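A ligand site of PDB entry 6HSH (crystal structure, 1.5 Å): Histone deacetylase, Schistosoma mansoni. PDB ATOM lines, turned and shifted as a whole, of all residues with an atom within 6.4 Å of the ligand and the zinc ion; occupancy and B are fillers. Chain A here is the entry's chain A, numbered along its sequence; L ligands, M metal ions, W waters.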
ATOM      1  N   PHE A  22      19.170   7.786 -37.297  1.00  0.00           N
ATOM      2  CA  PHE A  22      20.240   6.802 -37.286  1.00  0.00           C
ATOM      3  C   PHE A  22      20.521   6.230 -38.673  1.00  0.00           C
ATOM      4  O   PHE A  22      21.428   5.412 -38.802  1.00  0.00           O
ATOM      5  CB  PHE A  22      19.933   5.673 -36.297  1.00  0.00           C
ATOM      6  CG  PHE A  22      20.027   6.115 -34.856  1.00  0.00           C
ATOM      7  CD1 PHE A  22      21.266   6.347 -34.280  1.00  0.00           C
ATOM      8  CD2 PHE A  22      18.888   6.337 -34.105  1.00  0.00           C
ATOM      9  CE1 PHE A  22      21.360   6.780 -32.976  1.00  0.00           C
ATOM     10  CE2 PHE A  22      18.981   6.770 -32.800  1.00  0.00           C
ATOM     11  CZ  PHE A  22      20.219   6.993 -32.229  1.00  0.00           C
ATOM     12  N   TYR A 100       9.347  17.171 -31.800  1.00  0.00           N
ATOM     13  CA  TYR A 100      10.695  17.728 -31.792  1.00  0.00           C
ATOM     14  C   TYR A 100      11.760  16.645 -31.896  1.00  0.00           C
ATOM     15  O   TYR A 100      12.194  16.275 -32.991  1.00  0.00           O
ATOM     16  CB  TYR A 100      10.929  18.566 -30.519  1.00  0.00           C
ATOM     17  CG  TYR A 100       9.881  19.628 -30.228  1.00  0.00           C
ATOM     18  CD1 TYR A 100       9.736  20.740 -31.056  1.00  0.00           C
ATOM     19  CD2 TYR A 100       9.064  19.531 -29.107  1.00  0.00           C
ATOM     20  CE1 TYR A 100       8.779  21.728 -30.778  1.00  0.00           C
ATOM     21  CE2 TYR A 100       8.096  20.509 -28.831  1.00  0.00           C
ATOM     22  CZ  TYR A 100       7.958  21.604 -29.671  1.00  0.00           C
ATOM     23  OH  TYR A 100       7.021  22.569 -29.400  1.00  0.00           O
ATOM     24  N   ASP A 101      12.188  16.141 -30.744  1.00  0.00           N
ATOM     25  CA  ASP A 101      13.284  15.182 -30.680  1.00  0.00           C
ATOM     26  C   ASP A 101      12.858  13.769 -31.034  1.00  0.00           C
ATOM     27  O   ASP A 101      13.719  12.954 -31.373  1.00  0.00           O
ATOM     28  CB  ASP A 101      13.877  15.216 -29.276  1.00  0.00           C
ATOM     29  CG  ASP A 101      14.226  16.621 -28.865  1.00  0.00           C
ATOM     30  OD1 ASP A 101      15.084  17.201 -29.570  1.00  0.00           O
ATOM     31  OD2 ASP A 101      13.633  17.139 -27.898  1.00  0.00           O
ATOM     32  N   HIS A 142      17.236   3.324 -24.213  1.00  0.00           N
ATOM     33  CA  HIS A 142      17.070   3.352 -22.755  1.00  0.00           C
ATOM     34  C   HIS A 142      16.248   4.537 -22.241  1.00  0.00           C
ATOM     35  O   HIS A 142      15.890   4.520 -21.057  1.00  0.00           O
ATOM     36  CB  HIS A 142      18.448   3.338 -22.053  1.00  0.00           C
ATOM     37  CG  HIS A 142      19.398   4.427 -22.474  1.00  0.00           C
ATOM     38  ND1 HIS A 142      20.596   4.630 -21.830  1.00  0.00           N
ATOM     39  CD2 HIS A 142      19.349   5.340 -23.470  1.00  0.00           C
ATOM     40  CE1 HIS A 142      21.247   5.629 -22.407  1.00  0.00           C
ATOM     41  NE2 HIS A 142      20.512   6.077 -23.407  1.00  0.00           N
ATOM     42  N   HIS A 143      15.914   5.532 -23.073  1.00  0.00           N
ATOM     43  CA  HIS A 143      15.228   6.729 -22.598  1.00  0.00           C
ATOM     44  C   HIS A 143      13.708   6.642 -22.628  1.00  0.00           C
ATOM     45  O   HIS A 143      13.039   7.447 -21.951  1.00  0.00           O
ATOM     46  CB  HIS A 143      15.643   7.947 -23.440  1.00  0.00           C
ATOM     47  CG  HIS A 143      17.075   8.351 -23.272  1.00  0.00           C
ATOM     48  ND1 HIS A 143      17.657   8.515 -22.029  1.00  0.00           N
ATOM     49  CD2 HIS A 143      18.019   8.683 -24.182  1.00  0.00           C
ATOM     50  CE1 HIS A 143      18.910   8.903 -22.195  1.00  0.00           C
ATOM     51  NE2 HIS A 143      19.157   9.018 -23.491  1.00  0.00           N
ATOM     52  N   SER A 150      11.370   9.774 -25.726  1.00  0.00           N
ATOM     53  CA  SER A 150      12.388  10.659 -25.185  1.00  0.00           C
ATOM     54  C   SER A 150      13.736  10.353 -25.813  1.00  0.00           C
ATOM     55  O   SER A 150      14.090   9.193 -25.979  1.00  0.00           O
ATOM     56  CB  SER A 150      12.495  10.481 -23.670  1.00  0.00           C
ATOM     57  OG  SER A 150      13.533  11.305 -23.170  1.00  0.00           O
ATOM     58  N   GLY A 151      14.508  11.401 -26.103  1.00  0.00           N
ATOM     59  CA  GLY A 151      15.891  11.166 -26.486  1.00  0.00           C
ATOM     60  C   GLY A 151      16.079  10.252 -27.690  1.00  0.00           C
ATOM     61  O   GLY A 151      17.004   9.434 -27.693  1.00  0.00           O
ATOM     62  N   PHE A 152      15.249  10.405 -28.707  1.00  0.00           N
ATOM     63  CA  PHE A 152      15.245   9.580 -29.917  1.00  0.00           C
ATOM     64  C   PHE A 152      14.782   8.141 -29.664  1.00  0.00           C
ATOM     65  O   PHE A 152      14.945   7.292 -30.547  1.00  0.00           O
ATOM     66  CB  PHE A 152      16.628   9.522 -30.618  1.00  0.00           C
ATOM     67  CG  PHE A 152      17.426  10.813 -30.552  1.00  0.00           C
ATOM     68  CD1 PHE A 152      16.828  12.041 -30.817  1.00  0.00           C
ATOM     69  CD2 PHE A 152      18.789  10.787 -30.259  1.00  0.00           C
ATOM     70  CE1 PHE A 152      17.563  13.220 -30.758  1.00  0.00           C
ATOM     71  CE2 PHE A 152      19.531  11.970 -30.211  1.00  0.00           C
ATOM     72  CZ  PHE A 152      18.906  13.185 -30.464  1.00  0.00           C
ATOM     73  N   CYS A 153      14.214   7.846 -28.497  1.00  0.00           N
ATOM     74  CA  CYS A 153      13.764   6.506 -28.131  1.00  0.00           C
ATOM     75  C   CYS A 153      12.251   6.497 -28.072  1.00  0.00           C
ATOM     76  O   CYS A 153      11.665   7.347 -27.396  1.00  0.00           O
ATOM     77  CB  CYS A 153      14.312   6.076 -26.761  1.00  0.00           C
ATOM     78  SG  CYS A 153      16.103   6.031 -26.643  1.00  0.00           S
ATOM     79  N   ASP A 187      26.320   3.943 -21.954  1.00  0.00           N
ATOM     80  CA  ASP A 187      26.067   5.091 -22.821  1.00  0.00           C
ATOM     81  C   ASP A 187      26.614   6.393 -22.223  1.00  0.00           C
ATOM     82  O   ASP A 187      26.728   6.547 -21.000  1.00  0.00           O
ATOM     83  CB  ASP A 187      24.550   5.243 -23.027  1.00  0.00           C
ATOM     84  CG  ASP A 187      24.184   6.063 -24.235  1.00  0.00           C
ATOM     85  OD1 ASP A 187      24.110   7.293 -24.109  1.00  0.00           O
ATOM     86  OD2 ASP A 187      23.897   5.477 -25.300  1.00  0.00           O
ATOM     87  N   LEU A 188      26.909   7.369 -23.092  1.00  0.00           N
ATOM     88  CA  LEU A 188      27.268   8.697 -22.621  1.00  0.00           C
ATOM     89  C   LEU A 188      26.175   9.309 -21.736  1.00  0.00           C
ATOM     90  O   LEU A 188      26.476  10.083 -20.819  1.00  0.00           O
ATOM     91  CB  LEU A 188      27.563   9.626 -23.792  1.00  0.00           C
ATOM     92  CG  LEU A 188      27.978  11.061 -23.434  1.00  0.00           C
ATOM     93  CD1 LEU A 188      29.337  11.075 -22.759  1.00  0.00           C
ATOM     94  CD2 LEU A 188      28.000  11.903 -24.709  1.00  0.00           C
ATOM     95  N   HIS A 189      24.923   8.971 -21.996  1.00  0.00           N
ATOM     96  CA  HIS A 189      23.832   9.598 -21.270  1.00  0.00           C
ATOM     97  C   HIS A 189      23.276   8.666 -20.194  1.00  0.00           C
ATOM     98  O   HIS A 189      23.384   7.438 -20.247  1.00  0.00           O
ATOM     99  CB  HIS A 189      22.721  10.025 -22.230  1.00  0.00           C
ATOM    100  CG  HIS A 189      23.212  10.925 -23.314  1.00  0.00           C
ATOM    101  ND1 HIS A 189      23.750  10.441 -24.484  1.00  0.00           N
ATOM    102  CD2 HIS A 189      23.315  12.275 -23.381  1.00  0.00           C
ATOM    103  CE1 HIS A 189      24.106  11.451 -25.258  1.00  0.00           C
ATOM    104  NE2 HIS A 189      23.867  12.576 -24.599  1.00  0.00           N
ATOM    105  N   HIS A 190      22.649   9.299 -19.198  1.00  0.00           N
ATOM    106  CA  HIS A 190      22.023   8.550 -18.104  1.00  0.00           C
ATOM    107  C   HIS A 190      20.887   7.668 -18.617  1.00  0.00           C
ATOM    108  O   HIS A 190      20.008   8.132 -19.345  1.00  0.00           O
ATOM    109  CB  HIS A 190      21.509   9.540 -17.061  1.00  0.00           C
ATOM    110  CG  HIS A 190      20.750   8.892 -15.949  1.00  0.00           C
ATOM    111  ND1 HIS A 190      19.461   9.253 -15.596  1.00  0.00           N
ATOM    112  CD2 HIS A 190      21.083   7.867 -15.122  1.00  0.00           C
ATOM    113  CE1 HIS A 190      19.060   8.504 -14.587  1.00  0.00           C
ATOM    114  NE2 HIS A 190      20.024   7.661 -14.270  1.00  0.00           N
ATOM    115  N   PHE A 217      21.479  16.539 -21.477  1.00  0.00           N
ATOM    116  CA  PHE A 217      20.411  15.522 -21.491  1.00  0.00           C
ATOM    117  C   PHE A 217      20.765  14.227 -20.741  1.00  0.00           C
ATOM    118  O   PHE A 217      21.890  13.767 -20.857  1.00  0.00           O
ATOM    119  CB  PHE A 217      20.070  15.192 -22.943  1.00  0.00           C
ATOM    120  CG  PHE A 217      18.851  14.336 -23.091  1.00  0.00           C
ATOM    121  CD1 PHE A 217      17.597  14.925 -23.075  1.00  0.00           C
ATOM    122  CD2 PHE A 217      18.962  12.964 -23.238  1.00  0.00           C
ATOM    123  CE1 PHE A 217      16.466  14.149 -23.206  1.00  0.00           C
ATOM    124  CE2 PHE A 217      17.833  12.175 -23.365  1.00  0.00           C
ATOM    125  CZ  PHE A 217      16.581  12.772 -23.345  1.00  0.00           C
ATOM    126  N   GLN A 282      24.020  -2.035 -21.804  1.00  0.00           N
ATOM    127  CA  GLN A 282      23.768  -1.076 -22.875  1.00  0.00           C
ATOM    128  C   GLN A 282      25.121  -0.484 -23.244  1.00  0.00           C
ATOM    129  O   GLN A 282      25.866  -0.019 -22.362  1.00  0.00           O
ATOM    130  CB  GLN A 282      22.772   0.008 -22.422  1.00  0.00           C
ATOM    131  CG  GLN A 282      22.075   0.801 -23.549  1.00  0.00           C
ATOM    132  CD  GLN A 282      22.868   2.045 -23.961  1.00  0.00           C
ATOM    133  OE1 GLN A 282      24.064   2.153 -23.658  1.00  0.00           O
ATOM    134  NE2 GLN A 282      22.197   2.997 -24.636  1.00  0.00           N
ATOM    135  N   GLY A 284      25.977   1.967 -25.707  1.00  0.00           N
ATOM    136  CA  GLY A 284      25.926   3.163 -26.528  1.00  0.00           C
ATOM    137  C   GLY A 284      27.319   3.682 -26.809  1.00  0.00           C
ATOM    138  O   GLY A 284      28.151   3.748 -25.907  1.00  0.00           O
ATOM    139  N   ASP A 286      28.435   6.641 -27.834  1.00  0.00           N
ATOM    140  CA  ASP A 286      28.666   8.075 -27.859  1.00  0.00           C
ATOM    141  C   ASP A 286      29.687   8.550 -26.835  1.00  0.00           C
ATOM    142  O   ASP A 286      29.943   9.757 -26.758  1.00  0.00           O
ATOM    143  CB  ASP A 286      27.346   8.856 -27.713  1.00  0.00           C
ATOM    144  CG  ASP A 286      26.346   8.204 -26.763  1.00  0.00           C
ATOM    145  OD1 ASP A 286      26.682   7.266 -26.019  1.00  0.00           O
ATOM    146  OD2 ASP A 286      25.199   8.691 -26.780  1.00  0.00           O
ATOM    147  N   HIS A 293      29.375  14.367 -30.253  1.00  0.00           N
ATOM    148  CA  HIS A 293      29.260  14.922 -28.906  1.00  0.00           C
ATOM    149  C   HIS A 293      30.611  15.399 -28.395  1.00  0.00           C
ATOM    150  O   HIS A 293      30.723  16.493 -27.821  1.00  0.00           O
ATOM    151  CB  HIS A 293      28.685  13.896 -27.926  1.00  0.00           C
ATOM    152  CG  HIS A 293      27.198  13.743 -27.993  1.00  0.00           C
ATOM    153  ND1 HIS A 293      26.582  12.820 -28.819  1.00  0.00           N
ATOM    154  CD2 HIS A 293      26.204  14.372 -27.321  1.00  0.00           C
ATOM    155  CE1 HIS A 293      25.277  12.911 -28.663  1.00  0.00           C
ATOM    156  NE2 HIS A 293      25.013  13.835 -27.763  1.00  0.00           N
ATOM    157  N   GLY A 339      22.648   1.326 -28.678  1.00  0.00           N
ATOM    158  CA  GLY A 339      22.251   2.587 -28.081  1.00  0.00           C
ATOM    159  C   GLY A 339      22.740   3.755 -28.893  1.00  0.00           C
ATOM    160  O   GLY A 339      22.777   3.678 -30.133  1.00  0.00           O
ATOM    161  N   GLY A 340      23.133   4.830 -28.230  1.00  0.00           N
ATOM    162  CA  GLY A 340      23.695   5.998 -28.909  1.00  0.00           C
ATOM    163  C   GLY A 340      24.932   5.657 -29.724  1.00  0.00           C
ATOM    164  O   GLY A 340      25.513   4.575 -29.669  1.00  0.00           O
ATOM    165  N   GLY A 341      25.332   6.641 -30.527  1.00  0.00           N
ATOM    166  CA  GLY A 341      26.484   6.512 -31.397  1.00  0.00           C
ATOM    167  C   GLY A 341      26.214   7.211 -32.705  1.00  0.00           C
ATOM    168  O   GLY A 341      25.526   6.674 -33.575  1.00  0.00           O
ATOM    169  N   TYR A 342      26.735   8.427 -32.853  1.00  0.00           N
ATOM    170  CA  TYR A 342      26.363   9.300 -33.945  1.00  0.00           C
ATOM    171  C   TYR A 342      27.471   9.454 -34.974  1.00  0.00           C
ATOM    172  O   TYR A 342      27.268  10.112 -36.005  1.00  0.00           O
ATOM    173  CB  TYR A 342      25.899  10.642 -33.353  1.00  0.00           C
ATOM    174  CG  TYR A 342      24.828  10.331 -32.317  1.00  0.00           C
ATOM    175  CD1 TYR A 342      23.501  10.150 -32.703  1.00  0.00           C
ATOM    176  CD2 TYR A 342      25.162  10.120 -30.980  1.00  0.00           C
ATOM    177  CE1 TYR A 342      22.523   9.799 -31.770  1.00  0.00           C
ATOM    178  CE2 TYR A 342      24.196   9.777 -30.044  1.00  0.00           C
ATOM    179  CZ  TYR A 342      22.885   9.624 -30.444  1.00  0.00           C
ATOM    180  OH  TYR A 342      21.938   9.291 -29.511  1.00  0.00           O
HETATM  181  N1  LIG L   1      20.815   9.430 -25.546  1.00  0.00           N
HETATM  182  O1  LIG L   1      22.332   9.827 -27.157  1.00  0.00           O
HETATM  183  C1  LIG L   1      19.588  13.976 -26.827  1.00  0.00           C
HETATM  184  C2  LIG L   1      20.691  11.500 -26.755  1.00  0.00           C
HETATM  185  C3  LIG L   1      21.425  12.657 -26.960  1.00  0.00           C
HETATM  186  C4  LIG L   1      19.908  16.414 -26.489  1.00  0.00           C
HETATM  187  N2  LIG L   1      19.070  15.214 -26.611  1.00  0.00           N
HETATM  188  C5  LIG L   1      17.633  15.488 -26.463  1.00  0.00           C
HETATM  189  C6  LIG L   1      16.720  20.646 -32.595  1.00  0.00           C
HETATM  190  C7  LIG L   1      21.341  10.171 -26.529  1.00  0.00           C
HETATM  191  O2  LIG L   1      21.434   8.276 -25.078  1.00  0.00           O
HETATM  192  N3  LIG L   1      18.747  12.938 -26.688  1.00  0.00           N
HETATM  193  C8  LIG L   1      19.323  11.731 -26.654  1.00  0.00           C
HETATM  194  N4  LIG L   1      20.911  13.899 -26.993  1.00  0.00           N
HETATM  195  C9  LIG L   1      19.479  17.485 -27.486  1.00  0.00           C
HETATM  196  C10 LIG L   1      17.177  16.568 -27.445  1.00  0.00           C
HETATM  197  C11 LIG L   1      18.008  17.844 -27.338  1.00  0.00           C
HETATM  198  C12 LIG L   1      17.608  18.838 -28.412  1.00  0.00           C
HETATM  199  N5  LIG L   1      16.183  19.174 -28.388  1.00  0.00           N
HETATM  200  C13 LIG L   1      15.852  20.468 -28.966  1.00  0.00           C
HETATM  201  C14 LIG L   1      16.431  20.686 -30.336  1.00  0.00           C
HETATM  202  N6  LIG L   1      17.798  21.284 -32.011  1.00  0.00           N
HETATM  203  C15 LIG L   1      17.600  21.302 -30.655  1.00  0.00           C
HETATM  204  C16 LIG L   1      15.845  20.257 -31.573  1.00  0.00           C
HETATM  205  C17 LIG L   1      14.662  19.605 -31.927  1.00  0.00           C
HETATM  206  C18 LIG L   1      14.389  19.338 -33.258  1.00  0.00           C
HETATM  207  C19 LIG L   1      15.274  19.722 -34.251  1.00  0.00           C
HETATM  208  C20 LIG L   1      16.457  20.379 -33.929  1.00  0.00           C
HETATM  209  C21 LIG L   1      18.952  21.830 -32.712  1.00  0.00           C
HETATM  210 ZN    ZN M   1      23.527   8.538 -25.614  1.00  0.00          ZN
HETATM  211  O   HOH W   1      20.448   5.793 -26.623  1.00  0.00           O
HETATM  212  O   HOH W   2      15.525  19.865 -25.769  1.00  0.00           O
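The zinc ion is bound by OD1 of Asp 187 (2.0 Å), OD2 of Asp 286 (2.0 Å), O2 of the ligand (2.2 Å), ND1 of His 189 (2.2 Å) and O1 of the ligand (2.3 Å).
The zinc ion has five donor atoms within binding distance.
Within 4 Å of the zinc ion: Asp 187, His 189 and Asp 286.
The nearest printed residue that does not touch the zinc ion is Gly 340 (4.2 Å).
Water W1 bridges NE2 of His 142 (3.2 Å) and N of Gly 340 (3.3 Å).
O of Tyr 100 touches C18 of the ligand, at 3.8 Å.
Gly 151 touches the ligand (CA to N3, 3.4 Å).
Phe 152 touches the ligand (CE2 to C8, 3.6 Å).
CD1 of Phe 217 touches C5 of the ligand, at 3.4 Å.
His 293 touches the ligand (NE2 to C3, 3.9 Å).
Hydrophobic or aromatic side chains within 4 Å of the ligand: His 142, His 143, Phe 152, His 189, Phe 217 and Tyr 342.
N of Leu 188 lies within hydrogen-bond range of OD1 of Asp 286 (2.9 Å).
OD2 of Asp 187 is in hydrogen-bond range of NE2 of Gln 282 (3.1 Å).
OD2 of Asp 187 sits at hydrogen-bond distance from N of Gly 340 (3.1 Å).
N of His 143 is in hydrogen-bond range of SG of Cys 153, at 3.6 Å.
The backbone carbonyl oxygen of Gly 151 is in hydrogen-bond range of the side-chain sulfur of Cys 153.
A ring nitrogen (NE2) of His 143 is in hydrogen-bond range of a ring nitrogen (NE2) of His 142, at 3.2 Å.
OH of Tyr 342 sits close to O1 of the ligand (2.4 Å).
A ring nitrogen (NE2) of His 142 sits close to an oxygen (O2) of the ligand (2.9 Å).
A nitrogen (N5) of the ligand is in salt-bridge range of the side-chain carboxylate (OD1) of Asp 101 (2.5 Å).
A ring nitrogen (NE2) of His 143 lies within hydrogen-bond range of a nitrogen (N1) of the ligand.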
